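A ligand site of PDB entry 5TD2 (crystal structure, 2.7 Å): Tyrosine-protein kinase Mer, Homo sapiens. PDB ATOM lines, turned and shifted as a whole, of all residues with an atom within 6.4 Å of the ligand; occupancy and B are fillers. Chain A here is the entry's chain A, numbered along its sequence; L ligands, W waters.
The backbone NH (N) of Met 98 lies within hydrogen-bond range of an oxygen (O4) of the ligand, 2.8 Å away.
The backbone carbonyl oxygen (O) of Pro 96 lies close to a nitrogen (N5) of the ligand, 3.0 Å away.
An oxygen (O1) of the ligand is in hydrogen-bond range of the side-chain amino group of Lys 43 (3.1 Å).
O of Gly 18 is in hydrogen-bond range of N of Val 25, at 2.8 Å.
The side-chain carboxylate (OD1) of Asp 165 lies within salt-bridge range of the side-chain amino group (NZ) of Lys 43 (3.97 Å).
The backbone NH (N) of Thr 105 is in hydrogen-bond range of the side-chain carboxylate (OD2) of Asp 102 (2.8 Å).
O of Asn 152 sits at hydrogen-bond distance from N of Ala 164, at 3.1 Å.
O of Val 25 sits at hydrogen-bond distance from N of Leu 17 (2.8 Å).
OD1 of Asn 152 sits close to OD2 of Asp 165, 3.3 Å away.
The side-chain hydroxyl of Tyr 100 sits at hydrogen-bond distance from the side-chain amino group of Lys 99, at 2.8 Å.
O of Ala 41 is in hydrogen-bond range of N of Leu 95 (2.7 Å).
The side-chain carboxylate of Asp 102 lies close to a sulfur (S2) of the ligand (3.7 Å).
The side-chain sulfur (SD) of Met 154 sits close to an oxygen (O2) of the ligand, 3.6 Å away.
Leu 17 touches the ligand.
Glu 19 touches the ligand.
CA of Gly 20 touches C2 of the ligand, 3.6 Å away.
Val 25 touches the ligand.
Ala 41 touches the ligand (CB to C10, 3.3 Å).
Met 74 touches the ligand (SD to C18, 3.4 Å).
Leu 95 touches the ligand (CD1 to C18, 3.5 Å).
Phe 97 touches the ligand (CA to O4, 3.6 Å).
O of Lys 99 touches C22 of the ligand, at 3.0 Å.
CA of Gly 101 touches C16 of the ligand (3.8 Å).
Arg 151 touches the ligand (O to C12, 3.97 Å).
CA of Asn 152 touches C12 of the ligand (3.6 Å).
Ala 164 touches the ligand (CB to C12, 3.7 Å).
Asp 165 touches the ligand (CB to O1, 3.5 Å).
Hydrophobic or aromatic side chains that line the ligand: Leu 17, Val 25, Ala 41, Met 74, Leu 95, Phe 97, Met 98, Met 154 and Ala 164.
Of the 30 residues printed, 19 come within 4 Å of the ligand.
Water W2 bridges O of Leu 17 (3.0 Å) and S2 of the ligand (3.4 Å).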
ATOM      1  N   ILE A  16      -4.799 -20.114  -3.835  1.00  0.00           N
ATOM      2  CA  ILE A  16      -4.625 -19.424  -2.558  1.00  0.00           C
ATOM      3  C   ILE A  16      -5.664 -19.947  -1.560  1.00  0.00           C
ATOM      4  O   ILE A  16      -6.824 -20.198  -1.924  1.00  0.00           O
ATOM      5  CB  ILE A  16      -4.761 -17.878  -2.707  1.00  0.00           C
ATOM      6  CG1 ILE A  16      -3.854 -17.326  -3.813  1.00  0.00           C
ATOM      7  CG2 ILE A  16      -4.461 -17.171  -1.389  1.00  0.00           C
ATOM      8  CD1 ILE A  16      -2.379 -17.361  -3.506  1.00  0.00           C
ATOM      9  N   LEU A  17      -5.236 -20.139  -0.313  1.00  0.00           N
ATOM     10  CA  LEU A  17      -6.113 -20.546   0.789  1.00  0.00           C
ATOM     11  C   LEU A  17      -6.394 -19.393   1.735  1.00  0.00           C
ATOM     12  O   LEU A  17      -7.525 -19.216   2.186  1.00  0.00           O
ATOM     13  CB  LEU A  17      -5.484 -21.705   1.561  1.00  0.00           C
ATOM     14  CG  LEU A  17      -5.222 -22.960   0.728  1.00  0.00           C
ATOM     15  CD1 LEU A  17      -4.474 -23.985   1.547  1.00  0.00           C
ATOM     16  CD2 LEU A  17      -6.526 -23.530   0.196  1.00  0.00           C
ATOM     17  N   GLY A  18      -5.358 -18.618   2.049  1.00  0.00           N
ATOM     18  CA  GLY A  18      -5.515 -17.410   2.858  1.00  0.00           C
ATOM     19  C   GLY A  18      -4.273 -16.547   2.781  1.00  0.00           C
ATOM     20  O   GLY A  18      -3.350 -16.851   2.038  1.00  0.00           O
ATOM     21  N   GLU A  19      -4.267 -15.478   3.576  1.00  0.00           N
ATOM     22  CA  GLU A  19      -3.128 -14.558   3.642  1.00  0.00           C
ATOM     23  C   GLU A  19      -2.538 -14.566   5.043  1.00  0.00           C
ATOM     24  O   GLU A  19      -3.226 -14.231   6.012  1.00  0.00           O
ATOM     25  CB  GLU A  19      -3.564 -13.139   3.280  1.00  0.00           C
ATOM     26  CG  GLU A  19      -3.937 -12.953   1.808  1.00  0.00           C
ATOM     27  CD  GLU A  19      -2.777 -13.242   0.859  1.00  0.00           C
ATOM     28  OE1 GLU A  19      -1.604 -12.992   1.218  1.00  0.00           O
ATOM     29  OE2 GLU A  19      -3.058 -13.724  -0.256  1.00  0.00           O
ATOM     30  N   GLY A  20      -1.270 -14.955   5.138  1.00  0.00           N
ATOM     31  CA  GLY A  20      -0.498 -14.845   6.366  1.00  0.00           C
ATOM     32  C   GLY A  20       0.146 -13.482   6.491  1.00  0.00           C
ATOM     33  O   GLY A  20      -0.139 -12.567   5.698  1.00  0.00           O
ATOM     34  N   GLU A  21       1.025 -13.351   7.475  1.00  0.00           N
ATOM     35  CA  GLU A  21       1.667 -12.077   7.806  1.00  0.00           C
ATOM     36  C   GLU A  21       2.691 -11.657   6.757  1.00  0.00           C
ATOM     37  O   GLU A  21       2.714 -10.496   6.340  1.00  0.00           O
ATOM     38  CB  GLU A  21       2.319 -12.153   9.196  1.00  0.00           C
ATOM     39  CG  GLU A  21       2.652 -10.805   9.803  1.00  0.00           C
ATOM     40  CD  GLU A  21       1.426  -9.936  10.030  1.00  0.00           C
ATOM     41  OE1 GLU A  21       0.528 -10.364  10.782  1.00  0.00           O
ATOM     42  OE2 GLU A  21       1.345  -8.839   9.440  1.00  0.00           O
ATOM     43  N   GLY A  23       3.046 -13.246   3.695  1.00  0.00           N
ATOM     44  CA  GLY A  23       2.582 -13.530   2.330  1.00  0.00           C
ATOM     45  C   GLY A  23       1.349 -14.410   2.261  1.00  0.00           C
ATOM     46  O   GLY A  23       0.598 -14.553   3.240  1.00  0.00           O
ATOM     47  N   VAL A  25      -0.809 -17.935   1.814  1.00  0.00           N
ATOM     48  CA  VAL A  25      -0.814 -19.366   2.084  1.00  0.00           C
ATOM     49  C   VAL A  25      -1.508 -20.027   0.900  1.00  0.00           C
ATOM     50  O   VAL A  25      -2.670 -19.720   0.603  1.00  0.00           O
ATOM     51  CB  VAL A  25      -1.529 -19.714   3.411  1.00  0.00           C
ATOM     52  CG1 VAL A  25      -1.437 -21.216   3.700  1.00  0.00           C
ATOM     53  CG2 VAL A  25      -0.941 -18.909   4.556  1.00  0.00           C
ATOM     54  N   VAL A  40      -1.110 -30.369   0.874  1.00  0.00           N
ATOM     55  CA  VAL A  40      -0.427 -29.554   1.887  1.00  0.00           C
ATOM     56  C   VAL A  40      -0.832 -28.095   1.776  1.00  0.00           C
ATOM     57  O   VAL A  40      -1.409 -27.677   0.775  1.00  0.00           O
ATOM     58  CB  VAL A  40       1.116 -29.668   1.782  1.00  0.00           C
ATOM     59  CG1 VAL A  40       1.553 -31.079   2.123  1.00  0.00           C
ATOM     60  CG2 VAL A  40       1.627 -29.258   0.400  1.00  0.00           C
ATOM     61  N   ALA A  41      -0.533 -27.347   2.840  1.00  0.00           N
ATOM     62  CA  ALA A  41      -0.609 -25.891   2.841  1.00  0.00           C
ATOM     63  C   ALA A  41       0.803 -25.345   2.844  1.00  0.00           C
ATOM     64  O   ALA A  41       1.673 -25.876   3.548  1.00  0.00           O
ATOM     65  CB  ALA A  41      -1.370 -25.411   4.071  1.00  0.00           C
ATOM     66  N   VAL A  42       1.040 -24.279   2.077  1.00  0.00           N
ATOM     67  CA  VAL A  42       2.367 -23.701   1.912  1.00  0.00           C
ATOM     68  C   VAL A  42       2.348 -22.189   2.166  1.00  0.00           C
ATOM     69  O   VAL A  42       1.884 -21.418   1.316  1.00  0.00           O
ATOM     70  CB  VAL A  42       2.911 -23.971   0.477  1.00  0.00           C
ATOM     71  CG1 VAL A  42       4.304 -23.369   0.290  1.00  0.00           C
ATOM     72  CG2 VAL A  42       2.934 -25.476   0.211  1.00  0.00           C
ATOM     73  N   LYS A  43       2.855 -21.781   3.337  1.00  0.00           N
ATOM     74  CA  LYS A  43       3.085 -20.339   3.607  1.00  0.00           C
ATOM     75  C   LYS A  43       4.305 -19.842   2.860  1.00  0.00           C
ATOM     76  O   LYS A  43       5.359 -20.464   2.944  1.00  0.00           O
ATOM     77  CB  LYS A  43       3.366 -20.040   5.087  1.00  0.00           C
ATOM     78  CG  LYS A  43       2.358 -20.476   6.106  1.00  0.00           C
ATOM     79  CD  LYS A  43       2.464 -19.561   7.329  1.00  0.00           C
ATOM     80  CE  LYS A  43       1.587 -20.042   8.464  1.00  0.00           C
ATOM     81  NZ  LYS A  43       2.169 -19.662   9.775  1.00  0.00           N
ATOM     82  N   MET A  74       0.121 -27.870  15.501  1.00  0.00           N
ATOM     83  CA  MET A  74       0.524 -28.051  14.120  1.00  0.00           C
ATOM     84  C   MET A  74       1.997 -28.412  14.023  1.00  0.00           C
ATOM     85  O   MET A  74       2.843 -27.821  14.710  1.00  0.00           O
ATOM     86  CB  MET A  74       0.227 -26.794  13.287  1.00  0.00           C
ATOM     87  CG  MET A  74       0.539 -26.975  11.812  1.00  0.00           C
ATOM     88  SD  MET A  74      -0.287 -25.780  10.763  1.00  0.00           S
ATOM     89  CE  MET A  74      -1.953 -26.457  10.743  1.00  0.00           C
ATOM     90  N   LEU A  95       3.110 -27.048   5.573  1.00  0.00           N
ATOM     91  CA  LEU A  95       2.300 -27.434   6.738  1.00  0.00           C
ATOM     92  C   LEU A  95       1.172 -28.380   6.287  1.00  0.00           C
ATOM     93  O   LEU A  95       0.851 -28.427   5.101  1.00  0.00           O
ATOM     94  CB  LEU A  95       1.692 -26.190   7.367  1.00  0.00           C
ATOM     95  CG  LEU A  95       2.666 -25.076   7.768  1.00  0.00           C
ATOM     96  CD1 LEU A  95       1.914 -23.806   8.143  1.00  0.00           C
ATOM     97  CD2 LEU A  95       3.561 -25.524   8.902  1.00  0.00           C
ATOM     98  N   PRO A  96       0.562 -29.139   7.224  1.00  0.00           N
ATOM     99  CA  PRO A  96      -0.546 -30.013   6.850  1.00  0.00           C
ATOM    100  C   PRO A  96      -1.790 -29.237   6.415  1.00  0.00           C
ATOM    101  O   PRO A  96      -2.074 -28.180   6.974  1.00  0.00           O
ATOM    102  CB  PRO A  96      -0.859 -30.795   8.133  1.00  0.00           C
ATOM    103  CG  PRO A  96       0.224 -30.464   9.097  1.00  0.00           C
ATOM    104  CD  PRO A  96       0.787 -29.152   8.676  1.00  0.00           C
ATOM    105  N   PHE A  97      -2.533 -29.783   5.447  1.00  0.00           N
ATOM    106  CA  PHE A  97      -3.788 -29.185   5.006  1.00  0.00           C
ATOM    107  C   PHE A  97      -4.911 -29.382   6.022  1.00  0.00           C
ATOM    108  O   PHE A  97      -5.273 -30.512   6.367  1.00  0.00           O
ATOM    109  CB  PHE A  97      -4.218 -29.780   3.665  1.00  0.00           C
ATOM    110  CG  PHE A  97      -5.363 -29.048   3.015  1.00  0.00           C
ATOM    111  CD1 PHE A  97      -5.137 -27.881   2.296  1.00  0.00           C
ATOM    112  CD2 PHE A  97      -6.670 -29.540   3.118  1.00  0.00           C
ATOM    113  CE1 PHE A  97      -6.185 -27.213   1.687  1.00  0.00           C
ATOM    114  CE2 PHE A  97      -7.722 -28.871   2.501  1.00  0.00           C
ATOM    115  CZ  PHE A  97      -7.475 -27.708   1.794  1.00  0.00           C
ATOM    116  N   MET A  98      -5.468 -28.261   6.466  1.00  0.00           N
ATOM    117  CA  MET A  98      -6.575 -28.198   7.411  1.00  0.00           C
ATOM    118  C   MET A  98      -7.853 -27.910   6.618  1.00  0.00           C
ATOM    119  O   MET A  98      -8.092 -26.758   6.245  1.00  0.00           O
ATOM    120  CB  MET A  98      -6.298 -27.068   8.411  1.00  0.00           C
ATOM    121  CG  MET A  98      -4.992 -27.201   9.169  1.00  0.00           C
ATOM    122  SD  MET A  98      -5.046 -28.526  10.386  1.00  0.00           S
ATOM    123  CE  MET A  98      -4.483 -29.926   9.421  1.00  0.00           C
ATOM    124  N   LYS A  99      -8.677 -28.923   6.377  1.00  0.00           N
ATOM    125  CA  LYS A  99      -9.740 -28.802   5.364  1.00  0.00           C
ATOM    126  C   LYS A  99     -10.908 -27.900   5.745  1.00  0.00           C
ATOM    127  O   LYS A  99     -11.572 -27.356   4.857  1.00  0.00           O
ATOM    128  CB  LYS A  99     -10.225 -30.175   4.833  1.00  0.00           C
ATOM    129  CG  LYS A  99     -11.664 -30.629   5.109  1.00  0.00           C
ATOM    130  CD  LYS A  99     -11.904 -31.970   4.445  1.00  0.00           C
ATOM    131  CE  LYS A  99     -13.380 -32.390   4.460  1.00  0.00           C
ATOM    132  NZ  LYS A  99     -13.758 -33.143   5.686  1.00  0.00           N
ATOM    133  N   TYR A 100     -11.144 -27.717   7.041  1.00  0.00           N
ATOM    134  CA  TYR A 100     -12.170 -26.767   7.502  1.00  0.00           C
ATOM    135  C   TYR A 100     -11.637 -25.364   7.836  1.00  0.00           C
ATOM    136  O   TYR A 100     -12.406 -24.495   8.222  1.00  0.00           O
ATOM    137  CB  TYR A 100     -12.914 -27.333   8.696  1.00  0.00           C
ATOM    138  CG  TYR A 100     -13.607 -28.637   8.424  1.00  0.00           C
ATOM    139  CD1 TYR A 100     -14.613 -28.723   7.472  1.00  0.00           C
ATOM    140  CD2 TYR A 100     -13.265 -29.787   9.113  1.00  0.00           C
ATOM    141  CE1 TYR A 100     -15.264 -29.920   7.219  1.00  0.00           C
ATOM    142  CE2 TYR A 100     -13.897 -30.989   8.874  1.00  0.00           C
ATOM    143  CZ  TYR A 100     -14.897 -31.048   7.922  1.00  0.00           C
ATOM    144  OH  TYR A 100     -15.539 -32.241   7.710  1.00  0.00           O
ATOM    145  N   GLY A 101     -10.330 -25.150   7.677  1.00  0.00           N
ATOM    146  CA  GLY A 101      -9.743 -23.827   7.809  1.00  0.00           C
ATOM    147  C   GLY A 101      -9.632 -23.371   9.243  1.00  0.00           C
ATOM    148  O   GLY A 101      -9.636 -24.172  10.170  1.00  0.00           O
ATOM    149  N   ASP A 102      -9.540 -22.050   9.432  1.00  0.00           N
ATOM    150  CA  ASP A 102      -9.450 -21.478  10.781  1.00  0.00           C
ATOM    151  C   ASP A 102     -10.771 -21.668  11.529  1.00  0.00           C
ATOM    152  O   ASP A 102     -11.831 -21.789  10.916  1.00  0.00           O
ATOM    153  CB  ASP A 102      -9.060 -20.008  10.746  1.00  0.00           C
ATOM    154  CG  ASP A 102     -10.134 -19.119  10.132  1.00  0.00           C
ATOM    155  OD1 ASP A 102     -10.142 -18.970   8.893  1.00  0.00           O
ATOM    156  OD2 ASP A 102     -10.944 -18.578  10.903  1.00  0.00           O
ATOM    157  N   THR A 105     -13.669 -18.555  11.424  1.00  0.00           N
ATOM    158  CA  THR A 105     -14.494 -18.570  10.218  1.00  0.00           C
ATOM    159  C   THR A 105     -15.449 -19.777  10.176  1.00  0.00           C
ATOM    160  O   THR A 105     -16.568 -19.656   9.679  1.00  0.00           O
ATOM    161  CB  THR A 105     -13.620 -18.565   8.950  1.00  0.00           C
ATOM    162  OG1 THR A 105     -12.733 -17.432   9.009  1.00  0.00           O
ATOM    163  CG2 THR A 105     -14.470 -18.465   7.692  1.00  0.00           C
ATOM    164  N   TYR A 109     -19.616 -19.534   9.872  1.00  0.00           N
ATOM    165  CA  TYR A 109     -20.420 -20.367   8.967  1.00  0.00           C
ATOM    166  C   TYR A 109     -21.458 -21.243   9.675  1.00  0.00           C
ATOM    167  O   TYR A 109     -22.513 -21.491   9.109  1.00  0.00           O
ATOM    168  CB  TYR A 109     -19.535 -21.285   8.100  1.00  0.00           C
ATOM    169  CG  TYR A 109     -18.666 -20.606   7.056  1.00  0.00           C
ATOM    170  CD1 TYR A 109     -19.075 -19.437   6.405  1.00  0.00           C
ATOM    171  CD2 TYR A 109     -17.443 -21.172   6.673  1.00  0.00           C
ATOM    172  CE1 TYR A 109     -18.273 -18.843   5.441  1.00  0.00           C
ATOM    173  CE2 TYR A 109     -16.647 -20.591   5.699  1.00  0.00           C
ATOM    174  CZ  TYR A 109     -17.058 -19.423   5.081  1.00  0.00           C
ATOM    175  OH  TYR A 109     -16.277 -18.833   4.124  1.00  0.00           O
ATOM    176  N   ARG A 151      -8.982 -17.407  15.133  1.00  0.00           N
ATOM    177  CA  ARG A 151      -8.454 -17.324  13.759  1.00  0.00           C
ATOM    178  C   ARG A 151      -7.136 -18.077  13.576  1.00  0.00           C
ATOM    179  O   ARG A 151      -6.821 -18.514  12.467  1.00  0.00           O
ATOM    180  CB  ARG A 151      -8.276 -15.860  13.331  1.00  0.00           C
ATOM    181  CG  ARG A 151      -7.180 -15.102  14.072  1.00  0.00           C
ATOM    182  CD  ARG A 151      -6.914 -13.733  13.480  1.00  0.00           C
ATOM    183  NE  ARG A 151      -5.723 -13.153  14.089  1.00  0.00           N
ATOM    184  CZ  ARG A 151      -5.684 -12.585  15.294  1.00  0.00           C
ATOM    185  NH1 ARG A 151      -6.766 -12.483  16.073  1.00  0.00           N
ATOM    186  NH2 ARG A 151      -4.524 -12.114  15.740  1.00  0.00           N
ATOM    187  N   ASN A 152      -6.354 -18.191  14.654  1.00  0.00           N
ATOM    188  CA  ASN A 152      -5.083 -18.944  14.661  1.00  0.00           C
ATOM    189  C   ASN A 152      -5.201 -20.412  15.067  1.00  0.00           C
ATOM    190  O   ASN A 152      -4.196 -21.110  15.139  1.00  0.00           O
ATOM    191  CB  ASN A 152      -4.054 -18.232  15.541  1.00  0.00           C
ATOM    192  CG  ASN A 152      -3.570 -16.911  14.958  1.00  0.00           C
ATOM    193  OD1 ASN A 152      -3.312 -16.815  13.752  1.00  0.00           O
ATOM    194  ND2 ASN A 152      -3.450 -15.894  15.789  1.00  0.00           N
ATOM    195  N   CYS A 153      -6.425 -20.891  15.312  1.00  0.00           N
ATOM    196  CA  CYS A 153      -6.691 -22.302  15.576  1.00  0.00           C
ATOM    197  C   CYS A 153      -7.280 -22.928  14.313  1.00  0.00           C
ATOM    198  O   CYS A 153      -8.251 -22.407  13.766  1.00  0.00           O
ATOM    199  CB  CYS A 153      -7.680 -22.467  16.739  1.00  0.00           C
ATOM    200  SG  CYS A 153      -7.078 -21.778  18.295  1.00  0.00           S
ATOM    201  N   MET A 154      -6.707 -24.037  13.865  1.00  0.00           N
ATOM    202  CA  MET A 154      -7.082 -24.661  12.596  1.00  0.00           C
ATOM    203  C   MET A 154      -7.810 -25.982  12.821  1.00  0.00           C
ATOM    204  O   MET A 154      -7.710 -26.579  13.884  1.00  0.00           O
ATOM    205  CB  MET A 154      -5.829 -24.885  11.738  1.00  0.00           C
ATOM    206  CG  MET A 154      -4.967 -23.646  11.496  1.00  0.00           C
ATOM    207  SD  MET A 154      -5.756 -22.338  10.512  1.00  0.00           S
ATOM    208  CE  MET A 154      -6.013 -23.164   8.949  1.00  0.00           C
ATOM    209  N   ALA A 164      -1.880 -22.989  15.980  1.00  0.00           N
ATOM    210  CA  ALA A 164      -0.976 -22.652  14.881  1.00  0.00           C
ATOM    211  C   ALA A 164      -0.505 -21.198  14.997  1.00  0.00           C
ATOM    212  O   ALA A 164      -0.980 -20.466  15.868  1.00  0.00           O
ATOM    213  CB  ALA A 164      -1.678 -22.894  13.557  1.00  0.00           C
ATOM    214  N   ASP A 165       0.411 -20.810  14.114  1.00  0.00           N
ATOM    215  CA  ASP A 165       0.942 -19.429  14.026  1.00  0.00           C
ATOM    216  C   ASP A 165       1.754 -18.980  15.247  1.00  0.00           C
ATOM    217  O   ASP A 165       1.262 -18.245  16.115  1.00  0.00           O
ATOM    218  CB  ASP A 165      -0.172 -18.409  13.701  1.00  0.00           C
ATOM    219  CG  ASP A 165       0.381 -17.028  13.378  1.00  0.00           C
ATOM    220  OD1 ASP A 165       1.277 -16.932  12.512  1.00  0.00           O
ATOM    221  OD2 ASP A 165      -0.071 -16.050  13.991  1.00  0.00           O
ATOM    222  N   PHE A 166       3.023 -19.378  15.234  1.00  0.00           N
ATOM    223  CA  PHE A 166       3.940 -19.197  16.350  1.00  0.00           C
ATOM    224  C   PHE A 166       4.934 -18.060  16.078  1.00  0.00           C
ATOM    225  O   PHE A 166       5.568 -17.999  15.016  1.00  0.00           O
ATOM    226  CB  PHE A 166       4.694 -20.504  16.594  1.00  0.00           C
ATOM    227  CG  PHE A 166       3.799 -21.721  16.647  1.00  0.00           C
ATOM    228  CD1 PHE A 166       3.000 -21.970  17.760  1.00  0.00           C
ATOM    229  CD2 PHE A 166       3.745 -22.609  15.580  1.00  0.00           C
ATOM    230  CE1 PHE A 166       2.173 -23.091  17.809  1.00  0.00           C
ATOM    231  CE2 PHE A 166       2.927 -23.724  15.626  1.00  0.00           C
ATOM    232  CZ  PHE A 166       2.135 -23.968  16.737  1.00  0.00           C
HETATM  233  C1  LIG L   1      -2.336 -18.016   8.919  1.00  0.00           C
HETATM  234  C2  LIG L   1      -2.706 -17.438   7.536  1.00  0.00           C
HETATM  235  C3  LIG L   1      -6.567 -18.931   6.636  1.00  0.00           C
HETATM  236  C4  LIG L   1      -6.921 -21.178   5.626  1.00  0.00           C
HETATM  237  C5  LIG L   1      -7.390 -22.435   5.006  1.00  0.00           C
HETATM  238  C6  LIG L   1      -8.397 -24.721   3.809  1.00  0.00           C
HETATM  239  C7  LIG L   1      -7.118 -24.738   4.333  1.00  0.00           C
HETATM  240  C8  LIG L   1      -6.582 -23.593   4.936  1.00  0.00           C
HETATM  241  C9  LIG L   1      -4.491 -24.569   5.875  1.00  0.00           C
HETATM  242  C10 LIG L   1      -3.251 -24.271   6.592  1.00  0.00           C
HETATM  243  C11 LIG L   1      -1.599 -23.222   7.480  1.00  0.00           C
HETATM  244  C12 LIG L   1      -3.196 -19.981  11.763  1.00  0.00           C
HETATM  245  S1  LIG L   1      -2.115 -20.326  10.353  1.00  0.00           S
HETATM  246  O1  LIG L   1      -0.843 -19.743  10.586  1.00  0.00           O
HETATM  247  O2  LIG L   1      -2.243 -21.696   9.999  1.00  0.00           O
HETATM  248  N1  LIG L   1      -2.791 -19.417   9.126  1.00  0.00           N
HETATM  249  O3  LIG L   1      -4.000 -17.886   7.133  1.00  0.00           O
HETATM  250  C13 LIG L   1      -4.108 -19.313   6.969  1.00  0.00           C
HETATM  251  C14 LIG L   1      -3.859 -20.024   8.296  1.00  0.00           C
HETATM  252  C15 LIG L   1      -5.493 -19.713   6.510  1.00  0.00           C
HETATM  253  S2  LIG L   1      -7.954 -19.811   5.990  1.00  0.00           S
HETATM  254  N2  LIG L   1      -5.701 -20.893   5.972  1.00  0.00           N
HETATM  255  C16 LIG L   1      -8.676 -22.431   4.472  1.00  0.00           C
HETATM  256  C17 LIG L   1      -9.185 -23.559   3.872  1.00  0.00           C
HETATM  257  N3  LIG L   1      -5.316 -23.546   5.537  1.00  0.00           N
HETATM  258  O4  LIG L   1      -4.723 -25.724   5.630  1.00  0.00           O
HETATM  259  N4  LIG L   1      -2.706 -23.085   6.755  1.00  0.00           N
HETATM  260  C18 LIG L   1      -1.456 -24.534   7.816  1.00  0.00           C
HETATM  261  N5  LIG L   1      -2.503 -25.195   7.273  1.00  0.00           N
HETATM  262  N6  LIG L   1     -10.487 -23.489   3.363  1.00  0.00           N
HETATM  263  C19 LIG L   1     -10.683 -22.910   2.011  1.00  0.00           C
HETATM  264  C20 LIG L   1     -12.151 -22.429   1.992  1.00  0.00           C
HETATM  265  O5  LIG L   1     -13.028 -23.506   2.378  1.00  0.00           O
HETATM  266  C21 LIG L   1     -12.825 -24.141   3.655  1.00  0.00           C
HETATM  267  C22 LIG L   1     -11.372 -24.621   3.713  1.00  0.00           C
HETATM  268  O   HOH W   1      -8.846 -16.378   6.734  1.00  0.00           O
HETATM  269  O   HOH W   2      -9.328 -17.544   3.869  1.00  0.00           O
